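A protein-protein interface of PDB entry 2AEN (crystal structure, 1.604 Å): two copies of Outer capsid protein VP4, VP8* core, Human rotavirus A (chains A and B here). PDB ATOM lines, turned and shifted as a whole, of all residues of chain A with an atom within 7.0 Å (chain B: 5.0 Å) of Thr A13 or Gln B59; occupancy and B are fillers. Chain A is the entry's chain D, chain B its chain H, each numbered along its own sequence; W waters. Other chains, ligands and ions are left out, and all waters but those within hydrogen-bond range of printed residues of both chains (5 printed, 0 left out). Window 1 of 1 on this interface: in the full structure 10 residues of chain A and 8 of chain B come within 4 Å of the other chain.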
ATOM      1  N   TYR A  10      12.266  20.312   1.117  1.00  0.00           N
ATOM      2  CA  TYR A  10      12.906  19.294   0.304  1.00  0.00           C
ATOM      3  C   TYR A  10      14.395  19.576   0.222  1.00  0.00           C
ATOM      4  O   TYR A  10      14.822  20.710   0.074  1.00  0.00           O
ATOM      5  CB  TYR A  10      12.294  19.297  -1.110  1.00  0.00           C
ATOM      6  CG  TYR A  10      10.862  18.867  -1.128  1.00  0.00           C
ATOM      7  CD1 TYR A  10       9.834  19.776  -0.965  1.00  0.00           C
ATOM      8  CD2 TYR A  10      10.527  17.546  -1.330  1.00  0.00           C
ATOM      9  CE1 TYR A  10       8.496  19.369  -0.970  1.00  0.00           C
ATOM     10  CE2 TYR A  10       9.221  17.130  -1.331  1.00  0.00           C
ATOM     11  CZ  TYR A  10       8.200  18.037  -1.156  1.00  0.00           C
ATOM     12  OH  TYR A  10       6.907  17.582  -1.152  1.00  0.00           O
ATOM     13  N   GLN A  11      15.195  18.525   0.257  1.00  0.00           N
ATOM     14  CA  GLN A  11      16.649  18.673   0.219  1.00  0.00           C
ATOM     15  C   GLN A  11      17.156  18.908  -1.214  1.00  0.00           C
ATOM     16  O   GLN A  11      16.398  18.726  -2.178  1.00  0.00           O
ATOM     17  CB  GLN A  11      17.299  17.462   0.882  1.00  0.00           C
ATOM     18  CG  GLN A  11      16.934  17.318   2.377  1.00  0.00           C
ATOM     19  CD  GLN A  11      17.199  18.603   3.140  1.00  0.00           C
ATOM     20  OE1 GLN A  11      18.361  19.051   3.237  1.00  0.00           O
ATOM     21  NE2 GLN A  11      16.119  19.250   3.637  1.00  0.00           N
ATOM     22  N   PRO A  12      18.405  19.398  -1.363  1.00  0.00           N
ATOM     23  CA  PRO A  12      18.911  19.695  -2.706  1.00  0.00           C
ATOM     24  C   PRO A  12      18.725  18.501  -3.639  1.00  0.00           C
ATOM     25  O   PRO A  12      18.893  17.364  -3.219  1.00  0.00           O
ATOM     26  CB  PRO A  12      20.386  19.977  -2.454  1.00  0.00           C
ATOM     27  CG  PRO A  12      20.379  20.625  -1.099  1.00  0.00           C
ATOM     28  CD  PRO A  12      19.374  19.809  -0.328  1.00  0.00           C
ATOM     29  N   THR A  13      18.406  18.793  -4.896  1.00  0.00           N
ATOM     30  CA  THR A  13      17.934  17.757  -5.818  1.00  0.00           C
ATOM     31  C   THR A  13      18.052  18.250  -7.233  1.00  0.00           C
ATOM     32  O   THR A  13      18.285  19.432  -7.447  1.00  0.00           O
ATOM     33  CB  THR A  13      16.466  17.330  -5.519  1.00  0.00           C
ATOM     34  OG1 THR A  13      16.190  16.053  -6.138  1.00  0.00           O
ATOM     35  CG2 THR A  13      15.449  18.353  -5.988  1.00  0.00           C
ATOM     36  N   THR A  14      17.873  17.334  -8.184  1.00  0.00           N
ATOM     37  CA  THR A  14      17.708  17.654  -9.597  1.00  0.00           C
ATOM     38  C   THR A  14      16.301  17.184  -9.981  1.00  0.00           C
ATOM     39  O   THR A  14      15.942  16.014  -9.757  1.00  0.00           O
ATOM     40  CB  THR A  14      18.770  16.967 -10.462  1.00  0.00           C
ATOM     41  OG1 THR A  14      20.075  17.421 -10.052  1.00  0.00           O
ATOM     42  CG2 THR A  14      18.579  17.306 -11.923  1.00  0.00           C
ATOM     43  N   PHE A  15      15.533  18.084 -10.587  1.00  0.00           N
ATOM     44  CA  PHE A  15      14.065  17.981 -10.627  1.00  0.00           C
ATOM     45  C   PHE A  15      13.620  18.623 -11.935  1.00  0.00           C
ATOM     46  O   PHE A  15      14.113  19.704 -12.307  1.00  0.00           O
ATOM     47  CB  PHE A  15      13.524  18.786  -9.421  1.00  0.00           C
ATOM     48  CG  PHE A  15      12.029  18.693  -9.153  1.00  0.00           C
ATOM     49  CD1 PHE A  15      11.256  17.596  -9.501  1.00  0.00           C
ATOM     50  CD2 PHE A  15      11.414  19.726  -8.458  1.00  0.00           C
ATOM     51  CE1 PHE A  15       9.896  17.550  -9.182  1.00  0.00           C
ATOM     52  CE2 PHE A  15      10.064  19.694  -8.150  1.00  0.00           C
ATOM     53  CZ  PHE A  15       9.304  18.606  -8.499  1.00  0.00           C
ATOM     54  N   LYS A  16      12.699  17.961 -12.622  1.00  0.00           N
ATOM     55  CA  LYS A  16      11.977  18.549 -13.743  1.00  0.00           C
ATOM     56  C   LYS A  16      10.637  18.985 -13.167  1.00  0.00           C
ATOM     57  O   LYS A  16       9.723  18.188 -13.073  1.00  0.00           O
ATOM     58  CB  LYS A  16      11.813  17.504 -14.830  1.00  0.00           C
ATOM     59  CG  LYS A  16      13.138  17.168 -15.481  1.00  0.00           C
ATOM     60  CD  LYS A  16      12.952  16.240 -16.645  1.00  0.00           C
ATOM     61  CE  LYS A  16      14.295  15.651 -17.085  1.00  0.00           C
ATOM     62  NZ  LYS A  16      14.207  14.928 -18.409  1.00  0.00           N
ATOM     63  N   PRO A  17      10.540  20.246 -12.717  1.00  0.00           N
ATOM     64  CA  PRO A  17       9.381  20.598 -11.877  1.00  0.00           C
ATOM     65  C   PRO A  17       8.037  20.640 -12.624  1.00  0.00           C
ATOM     66  O   PRO A  17       7.989  20.946 -13.822  1.00  0.00           O
ATOM     67  CB  PRO A  17       9.747  21.982 -11.315  1.00  0.00           C
ATOM     68  CG  PRO A  17      11.170  22.223 -11.689  1.00  0.00           C
ATOM     69  CD  PRO A  17      11.451  21.388 -12.900  1.00  0.00           C
ATOM     70  N   PRO A  18       6.933  20.341 -11.916  1.00  0.00           N
ATOM     71  CA  PRO A  18       5.638  20.394 -12.566  1.00  0.00           C
ATOM     72  C   PRO A  18       5.191  21.826 -12.834  1.00  0.00           C
ATOM     73  O   PRO A  18       5.550  22.731 -12.086  1.00  0.00           O
ATOM     74  CB  PRO A  18       4.708  19.761 -11.529  1.00  0.00           C
ATOM     75  CG  PRO A  18       5.326  20.077 -10.262  1.00  0.00           C
ATOM     76  CD  PRO A  18       6.805  20.002 -10.487  1.00  0.00           C
ATOM     77  N   LEU A  23       8.526  26.870  -6.743  1.00  0.00           N
ATOM     78  CA  LEU A  23       9.632  26.406  -5.910  1.00  0.00           C
ATOM     79  C   LEU A  23      10.145  27.620  -5.146  1.00  0.00           C
ATOM     80  O   LEU A  23      10.544  28.599  -5.760  1.00  0.00           O
ATOM     81  CB  LEU A  23      10.755  25.785  -6.748  1.00  0.00           C
ATOM     82  CG  LEU A  23      10.319  24.716  -7.751  1.00  0.00           C
ATOM     83  CD1 LEU A  23      11.543  24.120  -8.417  1.00  0.00           C
ATOM     84  CD2 LEU A  23       9.496  23.634  -7.053  1.00  0.00           C
ATOM     85  N   ILE A 139      16.077  21.478 -13.292  1.00  0.00           N
ATOM     86  CA  ILE A 139      16.753  22.391 -12.377  1.00  0.00           C
ATOM     87  C   ILE A 139      17.579  21.605 -11.387  1.00  0.00           C
ATOM     88  O   ILE A 139      17.097  20.639 -10.789  1.00  0.00           O
ATOM     89  CB  ILE A 139      15.730  23.366 -11.696  1.00  0.00           C
ATOM     90  CG1 ILE A 139      16.435  24.446 -10.867  1.00  0.00           C
ATOM     91  CG2 ILE A 139      14.652  22.629 -10.925  1.00  0.00           C
ATOM     92  CD1 ILE A 139      15.465  25.424 -10.231  1.00  0.00           C
ATOM     93  N   ILE A 140      18.849  21.998 -11.258  1.00  0.00           N
ATOM     94  CA  ILE A 140      19.733  21.465 -10.210  1.00  0.00           C
ATOM     95  C   ILE A 140      19.640  22.492  -9.102  1.00  0.00           C
ATOM     96  O   ILE A 140      20.111  23.631  -9.242  1.00  0.00           O
ATOM     97  CB  ILE A 140      21.170  21.343 -10.670  1.00  0.00           C
ATOM     98  CG1 ILE A 140      21.268  20.477 -11.925  1.00  0.00           C
ATOM     99  CG2 ILE A 140      22.028  20.791  -9.556  1.00  0.00           C
ATOM    100  CD1 ILE A 140      22.637  20.470 -12.507  1.00  0.00           C
ATOM    101  N   ILE A 141      19.025  22.094  -7.999  1.00  0.00           N
ATOM    102  CA  ILE A 141      18.751  22.984  -6.882  1.00  0.00           C
ATOM    103  C   ILE A 141      19.784  22.690  -5.781  1.00  0.00           C
ATOM    104  O   ILE A 141      19.805  21.587  -5.225  1.00  0.00           O
ATOM    105  CB  ILE A 141      17.308  22.773  -6.329  1.00  0.00           C
ATOM    106  CG1 ILE A 141      16.263  22.892  -7.434  1.00  0.00           C
ATOM    107  CG2 ILE A 141      16.996  23.792  -5.248  1.00  0.00           C
ATOM    108  CD1 ILE A 141      14.847  22.512  -6.984  1.00  0.00           C
ATOM    109  N   HIS A 142      20.616  23.686  -5.459  1.00  0.00           N
ATOM    110  CA  HIS A 142      21.748  23.517  -4.526  1.00  0.00           C
ATOM    111  C   HIS A 142      21.379  23.689  -3.033  1.00  0.00           C
ATOM    112  O   HIS A 142      22.202  23.420  -2.155  1.00  0.00           O
ATOM    113  CB  HIS A 142      22.891  24.509  -4.846  1.00  0.00           C
ATOM    114  CG  HIS A 142      23.527  24.332  -6.194  1.00  0.00           C
ATOM    115  ND1 HIS A 142      24.888  24.468  -6.380  1.00  0.00           N
ATOM    116  CD2 HIS A 142      23.003  24.093  -7.419  1.00  0.00           C
ATOM    117  CE1 HIS A 142      25.174  24.275  -7.660  1.00  0.00           C
ATOM    118  NE2 HIS A 142      24.048  24.034  -8.311  1.00  0.00           N
ATOM    119  N   SER A 143      20.159  24.155  -2.764  1.00  0.00           N
ATOM    120  CA  SER A 143      19.735  24.496  -1.410  1.00  0.00           C
ATOM    121  C   SER A 143      18.340  23.914  -1.168  1.00  0.00           C
ATOM    122  O   SER A 143      17.636  23.573  -2.114  1.00  0.00           O
ATOM    123  CB  SER A 143      19.702  26.016  -1.258  1.00  0.00           C
ATOM    124  OG  SER A 143      21.025  26.550  -1.279  1.00  0.00           O
ATOM    125  N   PHE A 145      14.364  23.610  -0.320  1.00  0.00           N
ATOM    126  CA  PHE A 145      13.282  24.383  -0.927  1.00  0.00           C
ATOM    127  C   PHE A 145      11.911  23.839  -0.529  1.00  0.00           C
ATOM    128  O   PHE A 145      11.776  22.735  -0.006  1.00  0.00           O
ATOM    129  CB  PHE A 145      13.414  24.413  -2.458  1.00  0.00           C
ATOM    130  CG  PHE A 145      13.242  23.074  -3.114  1.00  0.00           C
ATOM    131  CD1 PHE A 145      12.060  22.770  -3.736  1.00  0.00           C
ATOM    132  CD2 PHE A 145      14.278  22.144  -3.141  1.00  0.00           C
ATOM    133  CE1 PHE A 145      11.887  21.534  -4.350  1.00  0.00           C
ATOM    134  CE2 PHE A 145      14.104  20.888  -3.725  1.00  0.00           C
ATOM    135  CZ  PHE A 145      12.912  20.603  -4.337  1.00  0.00           C
ATOM    136  N   ILE A 147       7.571  23.756  -1.779  1.00  0.00           N
ATOM    137  CA  ILE A 147       6.717  23.703  -2.976  1.00  0.00           C
ATOM    138  C   ILE A 147       5.359  24.285  -2.627  1.00  0.00           C
ATOM    139  O   ILE A 147       4.715  23.841  -1.676  1.00  0.00           O
ATOM    140  CB  ILE A 147       6.579  22.260  -3.527  1.00  0.00           C
ATOM    141  CG1 ILE A 147       7.936  21.726  -3.973  1.00  0.00           C
ATOM    142  CG2 ILE A 147       5.610  22.251  -4.692  1.00  0.00           C
ATOM    143  CD1 ILE A 147       7.933  20.283  -4.504  1.00  0.00           C
ATOM    144  N   ASN B  57      20.889  13.072  -5.528  1.00  0.00           N
ATOM    145  CA  ASN B  57      19.475  13.128  -5.198  1.00  0.00           C
ATOM    146  C   ASN B  57      18.675  13.615  -6.411  1.00  0.00           C
ATOM    147  O   ASN B  57      18.939  14.701  -6.930  1.00  0.00           O
ATOM    148  CB  ASN B  57      19.296  14.047  -3.990  1.00  0.00           C
ATOM    149  CG  ASN B  57      17.873  14.095  -3.479  1.00  0.00           C
ATOM    150  OD1 ASN B  57      16.929  14.268  -4.249  1.00  0.00           O
ATOM    151  ND2 ASN B  57      17.722  14.032  -2.139  1.00  0.00           N
ATOM    152  N   ARG B  58      17.690  12.819  -6.833  1.00  0.00           N
ATOM    153  CA  ARG B  58      16.755  13.200  -7.896  1.00  0.00           C
ATOM    154  C   ARG B  58      15.320  13.080  -7.379  1.00  0.00           C
ATOM    155  O   ARG B  58      14.988  12.159  -6.620  1.00  0.00           O
ATOM    156  CB  ARG B  58      16.959  12.344  -9.154  1.00  0.00           C
ATOM    157  CG  ARG B  58      18.240  12.650  -9.860  1.00  0.00           C
ATOM    158  CD  ARG B  58      18.300  12.065 -11.224  1.00  0.00           C
ATOM    159  NE  ARG B  58      19.534  12.454 -11.873  1.00  0.00           N
ATOM    160  CZ  ARG B  58      19.863  12.102 -13.107  1.00  0.00           C
ATOM    161  NH1 ARG B  58      19.059  11.330 -13.819  1.00  0.00           N
ATOM    162  NH2 ARG B  58      21.013  12.517 -13.619  1.00  0.00           N
ATOM    163  N   GLN B  59      14.485  14.035  -7.799  1.00  0.00           N
ATOM    164  CA  GLN B  59      13.101  14.109  -7.376  1.00  0.00           C
ATOM    165  C   GLN B  59      12.175  13.874  -8.550  1.00  0.00           C
ATOM    166  O   GLN B  59      12.460  14.308  -9.699  1.00  0.00           O
ATOM    167  CB  GLN B  59      12.838  15.491  -6.795  1.00  0.00           C
ATOM    168  CG  GLN B  59      11.445  15.659  -6.160  1.00  0.00           C
ATOM    169  CD  GLN B  59      11.370  16.866  -5.230  1.00  0.00           C
ATOM    170  OE1 GLN B  59      12.347  17.208  -4.588  1.00  0.00           O
ATOM    171  NE2 GLN B  59      10.199  17.489  -5.134  1.00  0.00           N
ATOM    172  N   TYR B  60      11.062  13.189  -8.263  1.00  0.00           N
ATOM    173  CA  TYR B  60      10.076  12.809  -9.260  1.00  0.00           C
ATOM    174  C   TYR B  60       8.695  12.982  -8.676  1.00  0.00           C
ATOM    175  O   TYR B  60       8.510  12.906  -7.454  1.00  0.00           O
ATOM    176  CB  TYR B  60      10.251  11.335  -9.633  1.00  0.00           C
ATOM    177  CG  TYR B  60      11.679  10.974 -10.061  1.00  0.00           C
ATOM    178  CD1 TYR B  60      12.564  10.429  -9.160  1.00  0.00           C
ATOM    179  CD2 TYR B  60      12.131  11.211 -11.354  1.00  0.00           C
ATOM    180  CE1 TYR B  60      13.864  10.143  -9.491  1.00  0.00           C
ATOM    181  CE2 TYR B  60      13.449  10.886 -11.725  1.00  0.00           C
ATOM    182  CZ  TYR B  60      14.310  10.330 -10.768  1.00  0.00           C
ATOM    183  OH  TYR B  60      15.620  10.004 -11.058  1.00  0.00           O
ATOM    184  N   ILE B  61       7.717  13.181  -9.538  1.00  0.00           N
ATOM    185  CA  ILE B  61       6.323  13.082  -9.103  1.00  0.00           C
ATOM    186  C   ILE B  61       5.786  11.703  -9.441  1.00  0.00           C
ATOM    187  O   ILE B  61       5.761  11.314 -10.614  1.00  0.00           O
ATOM    188  CB  ILE B  61       5.482  14.171  -9.752  1.00  0.00           C
ATOM    189  CG1 ILE B  61       6.063  15.526  -9.344  1.00  0.00           C
ATOM    190  CG2 ILE B  61       4.006  14.020  -9.348  1.00  0.00           C
ATOM    191  CD1 ILE B  61       5.269  16.676  -9.747  1.00  0.00           C
ATOM    192  N   ASN B  66       5.397  14.173  -4.579  1.00  0.00           N
ATOM    193  CA  ASN B  66       6.815  14.483  -4.697  1.00  0.00           C
ATOM    194  C   ASN B  66       7.647  13.504  -3.900  1.00  0.00           C
ATOM    195  O   ASN B  66       7.491  13.393  -2.688  1.00  0.00           O
ATOM    196  CB  ASN B  66       7.094  15.876  -4.171  1.00  0.00           C
ATOM    197  CG  ASN B  66       6.715  16.952  -5.166  1.00  0.00           C
ATOM    198  OD1 ASN B  66       7.496  17.269  -6.073  1.00  0.00           O
ATOM    199  ND2 ASN B  66       5.543  17.532  -4.989  1.00  0.00           N
ATOM    200  N   LYS B  67       8.529  12.795  -4.588  1.00  0.00           N
ATOM    201  CA  LYS B  67       9.399  11.783  -3.952  1.00  0.00           C
ATOM    202  C   LYS B  67      10.855  11.949  -4.403  1.00  0.00           C
ATOM    203  O   LYS B  67      11.148  12.060  -5.610  1.00  0.00           O
ATOM    204  CB  LYS B  67       8.933  10.369  -4.310  1.00  0.00           C
ATOM    205  CG  LYS B  67       7.496  10.025  -3.924  1.00  0.00           C
ATOM    206  CD  LYS B  67       7.328   9.887  -2.405  1.00  0.00           C
ATOM    207  CE  LYS B  67       5.969   9.303  -2.039  1.00  0.00           C
ATOM    208  NZ  LYS B  67       5.648   9.525  -0.602  1.00  0.00           N
ATOM    209  N   GLN B  68      11.760  11.910  -3.439  1.00  0.00           N
ATOM    210  CA  GLN B  68      13.181  11.944  -3.731  1.00  0.00           C
ATOM    211  C   GLN B  68      13.835  10.574  -3.559  1.00  0.00           C
ATOM    212  O   GLN B  68      13.462   9.773  -2.682  1.00  0.00           O
ATOM    213  CB  GLN B  68      13.879  12.952  -2.833  1.00  0.00           C
ATOM    214  CG  GLN B  68      13.447  14.409  -3.052  1.00  0.00           C
ATOM    215  CD  GLN B  68      14.337  15.416  -2.327  1.00  0.00           C
ATOM    216  OE1 GLN B  68      14.400  16.595  -2.710  1.00  0.00           O
ATOM    217  NE2 GLN B  68      15.013  14.978  -1.280  1.00  0.00           N
HETATM  218  O   HOH W   1      21.487  14.506 -11.147  1.00  0.00           O
HETATM  219  O   HOH W   2      14.919  14.168 -11.565  1.00  0.00           O
HETATM  220  O   HOH W   3      20.924  16.528  -7.516  1.00  0.00           O
HETATM  221  O   HOH W   4      14.277  15.817   1.037  1.00  0.00           O
HETATM  222  O   HOH W   5      11.890  15.224 -12.149  1.00  0.00           O
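No position is printed for both chains. Of the 18 pairs that touch across the chains among the printed residues, none has its exchanged pair printed and touching as well.
N of Gln B59 sits at hydrogen-bond distance from OG1 of Thr A13 (3.1 Å). OD1 of Asn B57 sits at hydrogen-bond distance from OG1 of Thr A13 (2.7 Å). The backbone NH (N) of Thr A14 sits at hydrogen-bond distance from the backbone carbonyl oxygen (O) of Asn B57 (3.1 Å). O of Thr A14 sits at hydrogen-bond distance from N of Gln B59 (3.1 Å). The side-chain amide oxygen of Gln B68 lies close to the backbone carbonyl oxygen of Gln A11.
Thr A13 touches just these residues of chain B: Asn B57 (2.7 Å), Arg B58 (3.3 Å), Gln B59 (3.1 Å) and Gln B68 (3.6 Å). Ile A140 touches none of the printed residues of chain B. Ser A143 touches none of the printed residues of chain B. Printed residues of chain B within 4 Å of Ile A147: Gln B59 and Asn B66. Of chain A, only Tyr A10 (3.7 Å), Thr A13 (3.1 Å), Thr A14 (3.1 Å), Phe A15 (3.5 Å), Phe A145 (3.5 Å) and Ile A147 (3.7 Å) come within 4 Å of Gln B59. Of the printed residues of chain A, Ile B61 touches Pro A18 (3.4 Å). The nearest printed residue of chain A that does not touch Ile B61 is Phe A15 (4.3 Å).
Water W4 bridges NE2 of Gln B68 (2.6 Å) and N of Gln A11 (3.0 Å). Water W5 lies within hydrogen-bond range of O of Gln B59 (2.7 Å) and N of Lys A16 (2.9 Å). Water W3 bridges O of Asn B57 (2.8 Å) and OG1 of Thr A14 (2.8 Å). Water W2 bridges the backbone carbonyl oxygen of Thr A14 and the backbone carbonyl oxygen of Gln B59. Water W1 lies within hydrogen-bond range of the guanidinium group (NE) of Arg B58 (2.9 Å) and the side-chain hydroxyl (OG1) of Thr A14 (3.4 Å).
NE2 of Gln B68 sits close to ND2 of Asn B57, 3.0 Å away. The side-chain amide nitrogen (NE2) of Gln B59 is in hydrogen-bond range of the side-chain amide oxygen (OD1) of Asn B66, 2.9 Å away. The side-chain amide oxygen (OE1) of Gln B59 lies close to the side-chain amide oxygen (OE1) of Gln B68, 2.8 Å away. The backbone carbonyl oxygen of Thr A13 is in hydrogen-bond range of the backbone NH of Ile A141 (2.8 Å). The backbone NH (N) of Ile A139 sits at hydrogen-bond distance from the backbone carbonyl oxygen (O) of Phe A15, 2.8 Å away. The backbone carbonyl oxygen (O) of Phe A145 lies within hydrogen-bond range of the backbone NH (N) of Tyr A10 (2.7 Å).
Hydrophobic or aromatic side chains of chain A that line the printed part of chain B: Tyr A10, Phe A15, Pro A18, Phe A145 and Ile A147. Along chain A the printed residues that touch a printed residue of chain B span positions 10 to 147. Of the 8 printed residues of chain B, 6 touch a printed residue of chain A. Printed residues of chain B that touch a printed residue of chain A: Asn B57, Arg B58, Gln B59, Ile B61, Asn B66 and Gln B68. Hydrophobic or aromatic side chains of chain B within 4 Å of the printed part of chain A: Ile B61.
OE1 of Gln B59 touches CD2 of Tyr A10 (3.7 Å). CB of Asn B66 touches OH of Tyr A10 (3.5 Å). Tyr A10 touches Gln B68 (CB to OE1, 3.8 Å). Thr A13 touches Gln B68. Thr A14 touches Arg B58 (O to CA, 3.5 Å). Phe A15 touches Gln B59 (CD1 to O, 3.5 Å). Pro A18 touches Ile B61. Gln B59 touches Phe A145 (OE1 to CZ, 3.5 Å). Gln B59 touches Ile A147. Ile A147 touches Asn B66 (CD1 to OD1, 3.4 Å).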
